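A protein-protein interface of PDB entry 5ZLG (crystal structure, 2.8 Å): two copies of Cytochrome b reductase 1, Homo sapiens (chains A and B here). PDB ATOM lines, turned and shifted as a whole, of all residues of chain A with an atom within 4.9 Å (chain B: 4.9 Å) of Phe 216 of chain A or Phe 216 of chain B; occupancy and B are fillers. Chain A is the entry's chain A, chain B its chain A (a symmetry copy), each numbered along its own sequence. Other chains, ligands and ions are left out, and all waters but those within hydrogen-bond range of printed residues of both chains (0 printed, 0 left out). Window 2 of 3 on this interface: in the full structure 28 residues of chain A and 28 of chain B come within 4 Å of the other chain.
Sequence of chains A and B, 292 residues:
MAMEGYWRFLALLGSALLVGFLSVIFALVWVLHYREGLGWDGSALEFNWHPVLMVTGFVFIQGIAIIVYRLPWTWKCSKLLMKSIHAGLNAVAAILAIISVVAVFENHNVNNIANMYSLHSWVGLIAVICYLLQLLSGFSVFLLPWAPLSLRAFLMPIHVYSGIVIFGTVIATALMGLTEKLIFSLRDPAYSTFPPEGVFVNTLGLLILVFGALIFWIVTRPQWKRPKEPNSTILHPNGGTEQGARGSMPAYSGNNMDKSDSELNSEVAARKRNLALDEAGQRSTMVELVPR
Of chain B, only Tyr 161 (3.5 Å) and Phe 216 (3.7 Å) come within 4 Å of Phe 216 of chain A.
Phe 216 of chain B touches just these residues of chain A: Tyr 161 and Phe 216.
Of the printed residues of chain A, Ala 213 of chain B touches Tyr 161 (2.8 Å).
Printed residues of chain B within 4 Å of Ala 213 of chain A: Tyr 161.
Of the printed residues of chain A, Tyr 161 of chain B touches Ala 213, Phe 216 and Trp 217.
Gly 212 of chain A touches none of the printed residues of chain B.
Ile 215 of chain B touches none of the printed residues of chain A.
Tyr 161 of chain A touches Ala 213 of chain B, and with the chains exchanged Ala 213 of chain A touches Tyr 161 of chain B.
Tyr 161 of chain A touches Phe 216 of chain B, and with the chains exchanged Phe 216 of chain A touches Tyr 161 of chain B.
Tyr 161 of chain A touches Trp 217 of chain B, and with the chains exchanged Trp 217 of chain A touches Tyr 161 of chain B.
Phe 216 of chain A touches its own counterpart, Phe 216 of chain B.
Of the 7 pairs that touch across the chains among the printed residues, 7 have their exchanged pair printed and touching as well.
Hydrophobic or aromatic side chains of chain B that line the printed part of chain A: Tyr 161, Ala 213, Phe 216 and Trp 217.
Printed residues of chain A that touch a printed residue of chain B: Tyr 161, Ala 213, Phe 216 and Trp 217.
Hydrophobic or aromatic side chains of chain A that line the printed part of chain B: Tyr 161, Ala 213, Phe 216 and Trp 217.
Among the printed residues, 7 pairs touch across the chains.
O of Ala 213 of chain A sits at hydrogen-bond distance from OH of Tyr 161 of chain B, 2.8 Å away.
OH of Tyr 161 of chain A sits at hydrogen-bond distance from O of Ala 213 of chain B (2.8 Å).
The backbone carbonyl oxygen of Trp 217 of chain A is in hydrogen-bond range of the guanidinium group of Arg 221 of chain A (3.0 Å).
O of Trp 217 of chain B is in hydrogen-bond range of NE of Arg 221 of chain B, at 3.0 Å.
O of Phe 216 of chain A lies within hydrogen-bond range of OG1 of Thr 220 of chain A, at 3.0 Å.
The backbone carbonyl oxygen (O) of Trp 217 of chain A lies within hydrogen-bond range of the side-chain hydroxyl (OG1) of Thr 220 of chain A (3.4 Å).
O of Trp 217 of chain B lies within hydrogen-bond range of OG1 of Thr 220 of chain B (3.4 Å).
The side-chain hydroxyl (OG1) of Thr 220 of chain B is in hydrogen-bond range of the backbone carbonyl oxygen (O) of Phe 216 of chain B (3.0 Å).
Phe 216 of chain B touches Tyr 161 of chain A.
Tyr 161 of chain A touches Trp 217 of chain B.
Tyr 161 of chain B touches Phe 216 of chain A.
Phe 216 of chain A touches Phe 216 of chain B.
Trp 217 of chain A touches Tyr 161 of chain B.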
ATOM      1  N   TYR A 161      14.209  -4.840 -14.122  1.00  0.00           N
ATOM      2  CA  TYR A 161      15.444  -5.019 -13.363  1.00  0.00           C
ATOM      3  C   TYR A 161      15.976  -3.677 -12.865  1.00  0.00           C
ATOM      4  O   TYR A 161      16.228  -3.488 -11.671  1.00  0.00           O
ATOM      5  CB  TYR A 161      16.473  -5.736 -14.245  1.00  0.00           C
ATOM      6  CG  TYR A 161      17.915  -5.621 -13.795  1.00  0.00           C
ATOM      7  CD1 TYR A 161      18.775  -4.726 -14.405  1.00  0.00           C
ATOM      8  CD2 TYR A 161      18.408  -6.403 -12.764  1.00  0.00           C
ATOM      9  CE1 TYR A 161      20.084  -4.603 -14.004  1.00  0.00           C
ATOM     10  CE2 TYR A 161      19.711  -6.279 -12.334  1.00  0.00           C
ATOM     11  CZ  TYR A 161      20.548  -5.381 -12.971  1.00  0.00           C
ATOM     12  OH  TYR A 161      21.857  -5.250 -12.567  1.00  0.00           O
ATOM     13  N   ILE A 164      14.090  -2.210  -9.975  1.00  0.00           N
ATOM     14  CA  ILE A 164      14.394  -2.826  -8.688  1.00  0.00           C
ATOM     15  C   ILE A 164      15.787  -2.416  -8.205  1.00  0.00           C
ATOM     16  O   ILE A 164      15.999  -2.158  -7.009  1.00  0.00           O
ATOM     17  CB  ILE A 164      14.244  -4.347  -8.808  1.00  0.00           C
ATOM     18  CG1 ILE A 164      12.902  -4.667  -9.485  1.00  0.00           C
ATOM     19  CG2 ILE A 164      14.397  -4.982  -7.445  1.00  0.00           C
ATOM     20  CD1 ILE A 164      12.241  -5.955  -9.024  1.00  0.00           C
ATOM     21  N   VAL A 165      16.747  -2.323  -9.131  1.00  0.00           N
ATOM     22  CA  VAL A 165      18.113  -1.962  -8.773  1.00  0.00           C
ATOM     23  C   VAL A 165      18.169  -0.538  -8.248  1.00  0.00           C
ATOM     24  O   VAL A 165      18.792  -0.273  -7.215  1.00  0.00           O
ATOM     25  CB  VAL A 165      19.052  -2.158  -9.977  1.00  0.00           C
ATOM     26  CG1 VAL A 165      20.147  -1.116  -9.975  1.00  0.00           C
ATOM     27  CG2 VAL A 165      19.653  -3.516  -9.929  1.00  0.00           C
ATOM     28  N   GLY A 212      11.712  -1.414   2.148  1.00  0.00           N
ATOM     29  CA  GLY A 212      12.298  -1.992   0.944  1.00  0.00           C
ATOM     30  C   GLY A 212      12.045  -3.488   0.820  1.00  0.00           C
ATOM     31  O   GLY A 212      11.688  -3.981  -0.256  1.00  0.00           O
ATOM     32  N   ALA A 213      12.228  -4.233   1.918  1.00  0.00           N
ATOM     33  CA  ALA A 213      12.043  -5.684   1.871  1.00  0.00           C
ATOM     34  C   ALA A 213      10.619  -6.047   1.474  1.00  0.00           C
ATOM     35  O   ALA A 213      10.399  -6.912   0.615  1.00  0.00           O
ATOM     36  CB  ALA A 213      12.383  -6.302   3.223  1.00  0.00           C
ATOM     37  N   LEU A 214       9.634  -5.396   2.101  1.00  0.00           N
ATOM     38  CA  LEU A 214       8.240  -5.642   1.758  1.00  0.00           C
ATOM     39  C   LEU A 214       7.980  -5.331   0.290  1.00  0.00           C
ATOM     40  O   LEU A 214       7.371  -6.132  -0.428  1.00  0.00           O
ATOM     41  CB  LEU A 214       7.323  -4.822   2.663  1.00  0.00           C
ATOM     42  CG  LEU A 214       7.349  -5.177   4.154  1.00  0.00           C
ATOM     43  CD1 LEU A 214       6.726  -4.089   4.990  1.00  0.00           C
ATOM     44  CD2 LEU A 214       6.642  -6.483   4.414  1.00  0.00           C
ATOM     45  N   ILE A 215       8.462  -4.186  -0.192  1.00  0.00           N
ATOM     46  CA  ILE A 215       8.188  -3.857  -1.585  1.00  0.00           C
ATOM     47  C   ILE A 215       8.830  -4.867  -2.527  1.00  0.00           C
ATOM     48  O   ILE A 215       8.278  -5.171  -3.596  1.00  0.00           O
ATOM     49  CB  ILE A 215       8.636  -2.421  -1.886  1.00  0.00           C
ATOM     50  CG1 ILE A 215       7.706  -1.435  -1.170  1.00  0.00           C
ATOM     51  CG2 ILE A 215       8.625  -2.162  -3.384  1.00  0.00           C
ATOM     52  CD1 ILE A 215       6.284  -1.461  -1.671  1.00  0.00           C
ATOM     53  N   PHE A 216       9.988  -5.425  -2.148  1.00  0.00           N
ATOM     54  CA  PHE A 216      10.636  -6.427  -2.999  1.00  0.00           C
ATOM     55  C   PHE A 216       9.862  -7.739  -2.997  1.00  0.00           C
ATOM     56  O   PHE A 216       9.662  -8.354  -4.057  1.00  0.00           O
ATOM     57  CB  PHE A 216      12.076  -6.655  -2.540  1.00  0.00           C
ATOM     58  CG  PHE A 216      12.903  -7.500  -3.489  1.00  0.00           C
ATOM     59  CD1 PHE A 216      13.145  -7.077  -4.793  1.00  0.00           C
ATOM     60  CD2 PHE A 216      13.462  -8.698  -3.069  1.00  0.00           C
ATOM     61  CE1 PHE A 216      13.900  -7.843  -5.659  1.00  0.00           C
ATOM     62  CE2 PHE A 216      14.233  -9.452  -3.931  1.00  0.00           C
ATOM     63  CZ  PHE A 216      14.447  -9.020  -5.226  1.00  0.00           C
ATOM     64  N   TRP A 217       9.412  -8.178  -1.818  1.00  0.00           N
ATOM     65  CA  TRP A 217       8.578  -9.369  -1.748  1.00  0.00           C
ATOM     66  C   TRP A 217       7.340  -9.217  -2.628  1.00  0.00           C
ATOM     67  O   TRP A 217       7.131  -9.998  -3.566  1.00  0.00           O
ATOM     68  CB  TRP A 217       8.178  -9.676  -0.298  1.00  0.00           C
ATOM     69  CG  TRP A 217       7.302 -10.886  -0.269  1.00  0.00           C
ATOM     70  CD1 TRP A 217       5.960 -10.898  -0.267  1.00  0.00           C
ATOM     71  CD2 TRP A 217       7.715 -12.262  -0.341  1.00  0.00           C
ATOM     72  NE1 TRP A 217       5.489 -12.187  -0.290  1.00  0.00           N
ATOM     73  CE2 TRP A 217       6.549 -13.045  -0.345  1.00  0.00           C
ATOM     74  CE3 TRP A 217       8.959 -12.907  -0.390  1.00  0.00           C
ATOM     75  CZ2 TRP A 217       6.580 -14.434  -0.391  1.00  0.00           C
ATOM     76  CZ3 TRP A 217       8.987 -14.301  -0.436  1.00  0.00           C
ATOM     77  CH2 TRP A 217       7.807 -15.042  -0.435  1.00  0.00           C
ATOM     78  N   ILE A 218       6.513  -8.201  -2.344  1.00  0.00           N
ATOM     79  CA  ILE A 218       5.323  -7.933  -3.161  1.00  0.00           C
ATOM     80  C   ILE A 218       5.668  -7.971  -4.645  1.00  0.00           C
ATOM     81  O   ILE A 218       5.036  -8.689  -5.430  1.00  0.00           O
ATOM     82  CB  ILE A 218       4.692  -6.578  -2.771  1.00  0.00           C
ATOM     83  CG1 ILE A 218       3.906  -6.680  -1.474  1.00  0.00           C
ATOM     84  CG2 ILE A 218       3.791  -6.060  -3.857  1.00  0.00           C
ATOM     85  CD1 ILE A 218       3.813  -5.361  -0.786  1.00  0.00           C
ATOM     86  N   VAL A 219       6.685  -7.211  -5.059  1.00  0.00           N
ATOM     87  CA  VAL A 219       6.944  -7.079  -6.489  1.00  0.00           C
ATOM     88  C   VAL A 219       7.578  -8.318  -7.116  1.00  0.00           C
ATOM     89  O   VAL A 219       7.727  -8.366  -8.344  1.00  0.00           O
ATOM     90  CB  VAL A 219       7.834  -5.854  -6.783  1.00  0.00           C
ATOM     91  CG1 VAL A 219       9.301  -6.212  -6.605  1.00  0.00           C
ATOM     92  CG2 VAL A 219       7.571  -5.328  -8.187  1.00  0.00           C
ATOM     93  N   THR A 220       7.964  -9.332  -6.337  1.00  0.00           N
ATOM     94  CA  THR A 220       8.500 -10.535  -6.970  1.00  0.00           C
ATOM     95  C   THR A 220       7.633 -11.765  -6.736  1.00  0.00           C
ATOM     96  O   THR A 220       8.121 -12.887  -6.753  1.00  0.00           O
ATOM     97  CB  THR A 220       9.930 -10.811  -6.517  1.00  0.00           C
ATOM     98  OG1 THR A 220       9.942 -11.103  -5.117  1.00  0.00           O
ATOM     99  CG2 THR A 220      10.800  -9.631  -6.831  1.00  0.00           C
ATOM    100  N   ARG A 221       6.345 -11.587  -6.512  1.00  0.00           N
ATOM    101  CA  ARG A 221       5.445 -12.724  -6.504  1.00  0.00           C
ATOM    102  C   ARG A 221       4.898 -12.882  -7.915  1.00  0.00           C
ATOM    103  O   ARG A 221       4.200 -11.976  -8.397  1.00  0.00           O
ATOM    104  CB  ARG A 221       4.318 -12.521  -5.509  1.00  0.00           C
ATOM    105  CG  ARG A 221       4.765 -12.433  -4.069  1.00  0.00           C
ATOM    106  CD  ARG A 221       5.791 -13.489  -3.717  1.00  0.00           C
ATOM    107  NE  ARG A 221       7.149 -12.966  -3.844  1.00  0.00           N
ATOM    108  CZ  ARG A 221       8.260 -13.685  -3.702  1.00  0.00           C
ATOM    109  NH1 ARG A 221       8.174 -14.969  -3.420  1.00  0.00           N
ATOM    110  NH2 ARG A 221       9.456 -13.113  -3.842  1.00  0.00           N
ATOM    111  N   TYR B 161      14.406 -15.556  -1.926  1.00  0.00           N
ATOM    112  CA  TYR B 161      14.156 -14.150  -1.623  1.00  0.00           C
ATOM    113  C   TYR B 161      15.098 -13.652  -0.528  1.00  0.00           C
ATOM    114  O   TYR B 161      15.801 -12.650  -0.691  1.00  0.00           O
ATOM    115  CB  TYR B 161      12.687 -13.982  -1.215  1.00  0.00           C
ATOM    116  CG  TYR B 161      12.358 -12.708  -0.463  1.00  0.00           C
ATOM    117  CD1 TYR B 161      12.206 -12.720   0.911  1.00  0.00           C
ATOM    118  CD2 TYR B 161      12.204 -11.503  -1.128  1.00  0.00           C
ATOM    119  CE1 TYR B 161      11.915 -11.573   1.610  1.00  0.00           C
ATOM    120  CE2 TYR B 161      11.934 -10.339  -0.443  1.00  0.00           C
ATOM    121  CZ  TYR B 161      11.778 -10.386   0.930  1.00  0.00           C
ATOM    122  OH  TYR B 161      11.494  -9.238   1.634  1.00  0.00           O
ATOM    123  N   ILE B 164      18.631 -13.065  -1.639  1.00  0.00           N
ATOM    124  CA  ILE B 164      18.824 -11.829  -2.390  1.00  0.00           C
ATOM    125  C   ILE B 164      18.734 -10.613  -1.465  1.00  0.00           C
ATOM    126  O   ILE B 164      19.503  -9.647  -1.601  1.00  0.00           O
ATOM    127  CB  ILE B 164      17.805 -11.767  -3.533  1.00  0.00           C
ATOM    128  CG1 ILE B 164      17.818 -13.104  -4.290  1.00  0.00           C
ATOM    129  CG2 ILE B 164      18.099 -10.573  -4.412  1.00  0.00           C
ATOM    130  CD1 ILE B 164      17.528 -13.003  -5.778  1.00  0.00           C
ATOM    131  N   VAL B 165      17.815 -10.654  -0.495  1.00  0.00           N
ATOM    132  CA  VAL B 165      17.632  -9.539   0.426  1.00  0.00           C
ATOM    133  C   VAL B 165      18.865  -9.355   1.293  1.00  0.00           C
ATOM    134  O   VAL B 165      19.354  -8.232   1.460  1.00  0.00           O
ATOM    135  CB  VAL B 165      16.368  -9.749   1.278  1.00  0.00           C
ATOM    136  CG1 VAL B 165      16.561  -9.185   2.666  1.00  0.00           C
ATOM    137  CG2 VAL B 165      15.207  -9.089   0.625  1.00  0.00           C
ATOM    138  N   GLY B 212      27.298  -6.013  -6.969  1.00  0.00           N
ATOM    139  CA  GLY B 212      25.941  -6.397  -6.598  1.00  0.00           C
ATOM    140  C   GLY B 212      24.984  -6.412  -7.781  1.00  0.00           C
ATOM    141  O   GLY B 212      24.194  -7.349  -7.944  1.00  0.00           O
ATOM    142  N   ALA B 213      25.037  -5.373  -8.625  1.00  0.00           N
ATOM    143  CA  ALA B 213      24.123  -5.293  -9.765  1.00  0.00           C
ATOM    144  C   ALA B 213      24.308  -6.475 -10.706  1.00  0.00           C
ATOM    145  O   ALA B 213      23.332  -7.103 -11.139  1.00  0.00           O
ATOM    146  CB  ALA B 213      24.335  -3.985 -10.520  1.00  0.00           C
ATOM    147  N   LEU B 214      25.564  -6.787 -11.040  1.00  0.00           N
ATOM    148  CA  LEU B 214      25.845  -7.930 -11.898  1.00  0.00           C
ATOM    149  C   LEU B 214      25.322  -9.218 -11.275  1.00  0.00           C
ATOM    150  O   LEU B 214      24.651 -10.015 -11.941  1.00  0.00           O
ATOM    151  CB  LEU B 214      27.344  -8.024 -12.175  1.00  0.00           C
ATOM    152  CG  LEU B 214      27.960  -6.869 -12.973  1.00  0.00           C
ATOM    153  CD1 LEU B 214      29.462  -6.859 -12.860  1.00  0.00           C
ATOM    154  CD2 LEU B 214      27.562  -6.941 -14.425  1.00  0.00           C
ATOM    155  N   ILE B 215      25.587  -9.432  -9.988  1.00  0.00           N
ATOM    156  CA  ILE B 215      25.126 -10.677  -9.388  1.00  0.00           C
ATOM    157  C   ILE B 215      23.606 -10.763  -9.395  1.00  0.00           C
ATOM    158  O   ILE B 215      23.037 -11.857  -9.536  1.00  0.00           O
ATOM    159  CB  ILE B 215      25.707 -10.829  -7.976  1.00  0.00           C
ATOM    160  CG1 ILE B 215      27.214 -11.097  -8.069  1.00  0.00           C
ATOM    161  CG2 ILE B 215      25.016 -11.964  -7.236  1.00  0.00           C
ATOM    162  CD1 ILE B 215      27.564 -12.408  -8.726  1.00  0.00           C
ATOM    163  N   PHE B 216      22.916  -9.622  -9.269  1.00  0.00           N
ATOM    164  CA  PHE B 216      21.451  -9.639  -9.300  1.00  0.00           C
ATOM    165  C   PHE B 216      20.930  -9.942 -10.700  1.00  0.00           C
ATOM    166  O   PHE B 216      19.997 -10.742 -10.865  1.00  0.00           O
ATOM    167  CB  PHE B 216      20.897  -8.305  -8.802  1.00  0.00           C
ATOM    168  CG  PHE B 216      19.398  -8.299  -8.579  1.00  0.00           C
ATOM    169  CD1 PHE B 216      18.813  -9.150  -7.646  1.00  0.00           C
ATOM    170  CD2 PHE B 216      18.579  -7.424  -9.279  1.00  0.00           C
ATOM    171  CE1 PHE B 216      17.447  -9.145  -7.438  1.00  0.00           C
ATOM    172  CE2 PHE B 216      17.217  -7.408  -9.055  1.00  0.00           C
ATOM    173  CZ  PHE B 216      16.657  -8.272  -8.135  1.00  0.00           C
ATOM    174  N   TRP B 217      21.529  -9.318 -11.719  1.00  0.00           N
ATOM    175  CA  TRP B 217      21.157  -9.631 -13.091  1.00  0.00           C
ATOM    176  C   TRP B 217      21.322 -11.123 -13.371  1.00  0.00           C
ATOM    177  O   TRP B 217      20.350 -11.813 -13.707  1.00  0.00           O
ATOM    178  CB  TRP B 217      21.978  -8.799 -14.086  1.00  0.00           C
ATOM    179  CG  TRP B 217      21.589  -9.167 -15.481  1.00  0.00           C
ATOM    180  CD1 TRP B 217      22.204 -10.063 -16.269  1.00  0.00           C
ATOM    181  CD2 TRP B 217      20.434  -8.717 -16.211  1.00  0.00           C
ATOM    182  NE1 TRP B 217      21.544 -10.185 -17.467  1.00  0.00           N
ATOM    183  CE2 TRP B 217      20.447  -9.373 -17.453  1.00  0.00           C
ATOM    184  CE3 TRP B 217      19.397  -7.813 -15.939  1.00  0.00           C
ATOM    185  CZ2 TRP B 217      19.474  -9.158 -18.424  1.00  0.00           C
ATOM    186  CZ3 TRP B 217      18.424  -7.600 -16.914  1.00  0.00           C
ATOM    187  CH2 TRP B 217      18.474  -8.269 -18.135  1.00  0.00           C
ATOM    188  N   ILE B 218      22.550 -11.638 -13.221  1.00  0.00           N
ATOM    189  CA  ILE B 218      22.806 -13.070 -13.413  1.00  0.00           C
ATOM    190  C   ILE B 218      21.760 -13.908 -12.686  1.00  0.00           C
ATOM    191  O   ILE B 218      21.116 -14.782 -13.279  1.00  0.00           O
ATOM    192  CB  ILE B 218      24.232 -13.433 -12.943  1.00  0.00           C
ATOM    193  CG1 ILE B 218      25.281 -13.004 -13.958  1.00  0.00           C
ATOM    194  CG2 ILE B 218      24.367 -14.908 -12.686  1.00  0.00           C
ATOM    195  CD1 ILE B 218      26.607 -12.785 -13.313  1.00  0.00           C
ATOM    196  N   VAL B 219      21.558 -13.650 -11.391  1.00  0.00           N
ATOM    197  CA  VAL B 219      20.697 -14.533 -10.611  1.00  0.00           C
ATOM    198  C   VAL B 219      19.210 -14.359 -10.906  1.00  0.00           C
ATOM    199  O   VAL B 219      18.396 -15.141 -10.396  1.00  0.00           O
ATOM    200  CB  VAL B 219      20.936 -14.350  -9.099  1.00  0.00           C
ATOM    201  CG1 VAL B 219      20.121 -13.179  -8.573  1.00  0.00           C
ATOM    202  CG2 VAL B 219      20.596 -15.629  -8.346  1.00  0.00           C
ATOM    203  N   THR B 220      18.803 -13.371 -11.707  1.00  0.00           N
ATOM    204  CA  THR B 220      17.382 -13.273 -12.030  1.00  0.00           C
ATOM    205  C   THR B 220      17.095 -13.483 -13.512  1.00  0.00           C
ATOM    206  O   THR B 220      16.107 -12.984 -14.034  1.00  0.00           O
ATOM    207  CB  THR B 220      16.799 -11.941 -11.570  1.00  0.00           C
ATOM    208  OG1 THR B 220      17.409 -10.872 -12.297  1.00  0.00           O
ATOM    209  CG2 THR B 220      17.004 -11.779 -10.094  1.00  0.00           C
ATOM    210  N   ARG B 221      17.941 -14.213 -14.214  1.00  0.00           N
ATOM    211  CA  ARG B 221      17.599 -14.624 -15.562  1.00  0.00           C
ATOM    212  C   ARG B 221      16.929 -15.986 -15.466  1.00  0.00           C
ATOM    213  O   ARG B 221      17.579 -16.951 -15.036  1.00  0.00           O
ATOM    214  CB  ARG B 221      18.834 -14.692 -16.440  1.00  0.00           C
ATOM    215  CG  ARG B 221      19.522 -13.365 -16.654  1.00  0.00           C
ATOM    216  CD  ARG B 221      18.543 -12.250 -16.956  1.00  0.00           C
ATOM    217  NE  ARG B 221      18.192 -11.518 -15.742  1.00  0.00           N
ATOM    218  CZ  ARG B 221      17.279 -10.552 -15.671  1.00  0.00           C
ATOM    219  NH1 ARG B 221      16.621 -10.195 -16.755  1.00  0.00           N
ATOM    220  NH2 ARG B 221      17.027  -9.946 -14.510  1.00  0.00           N
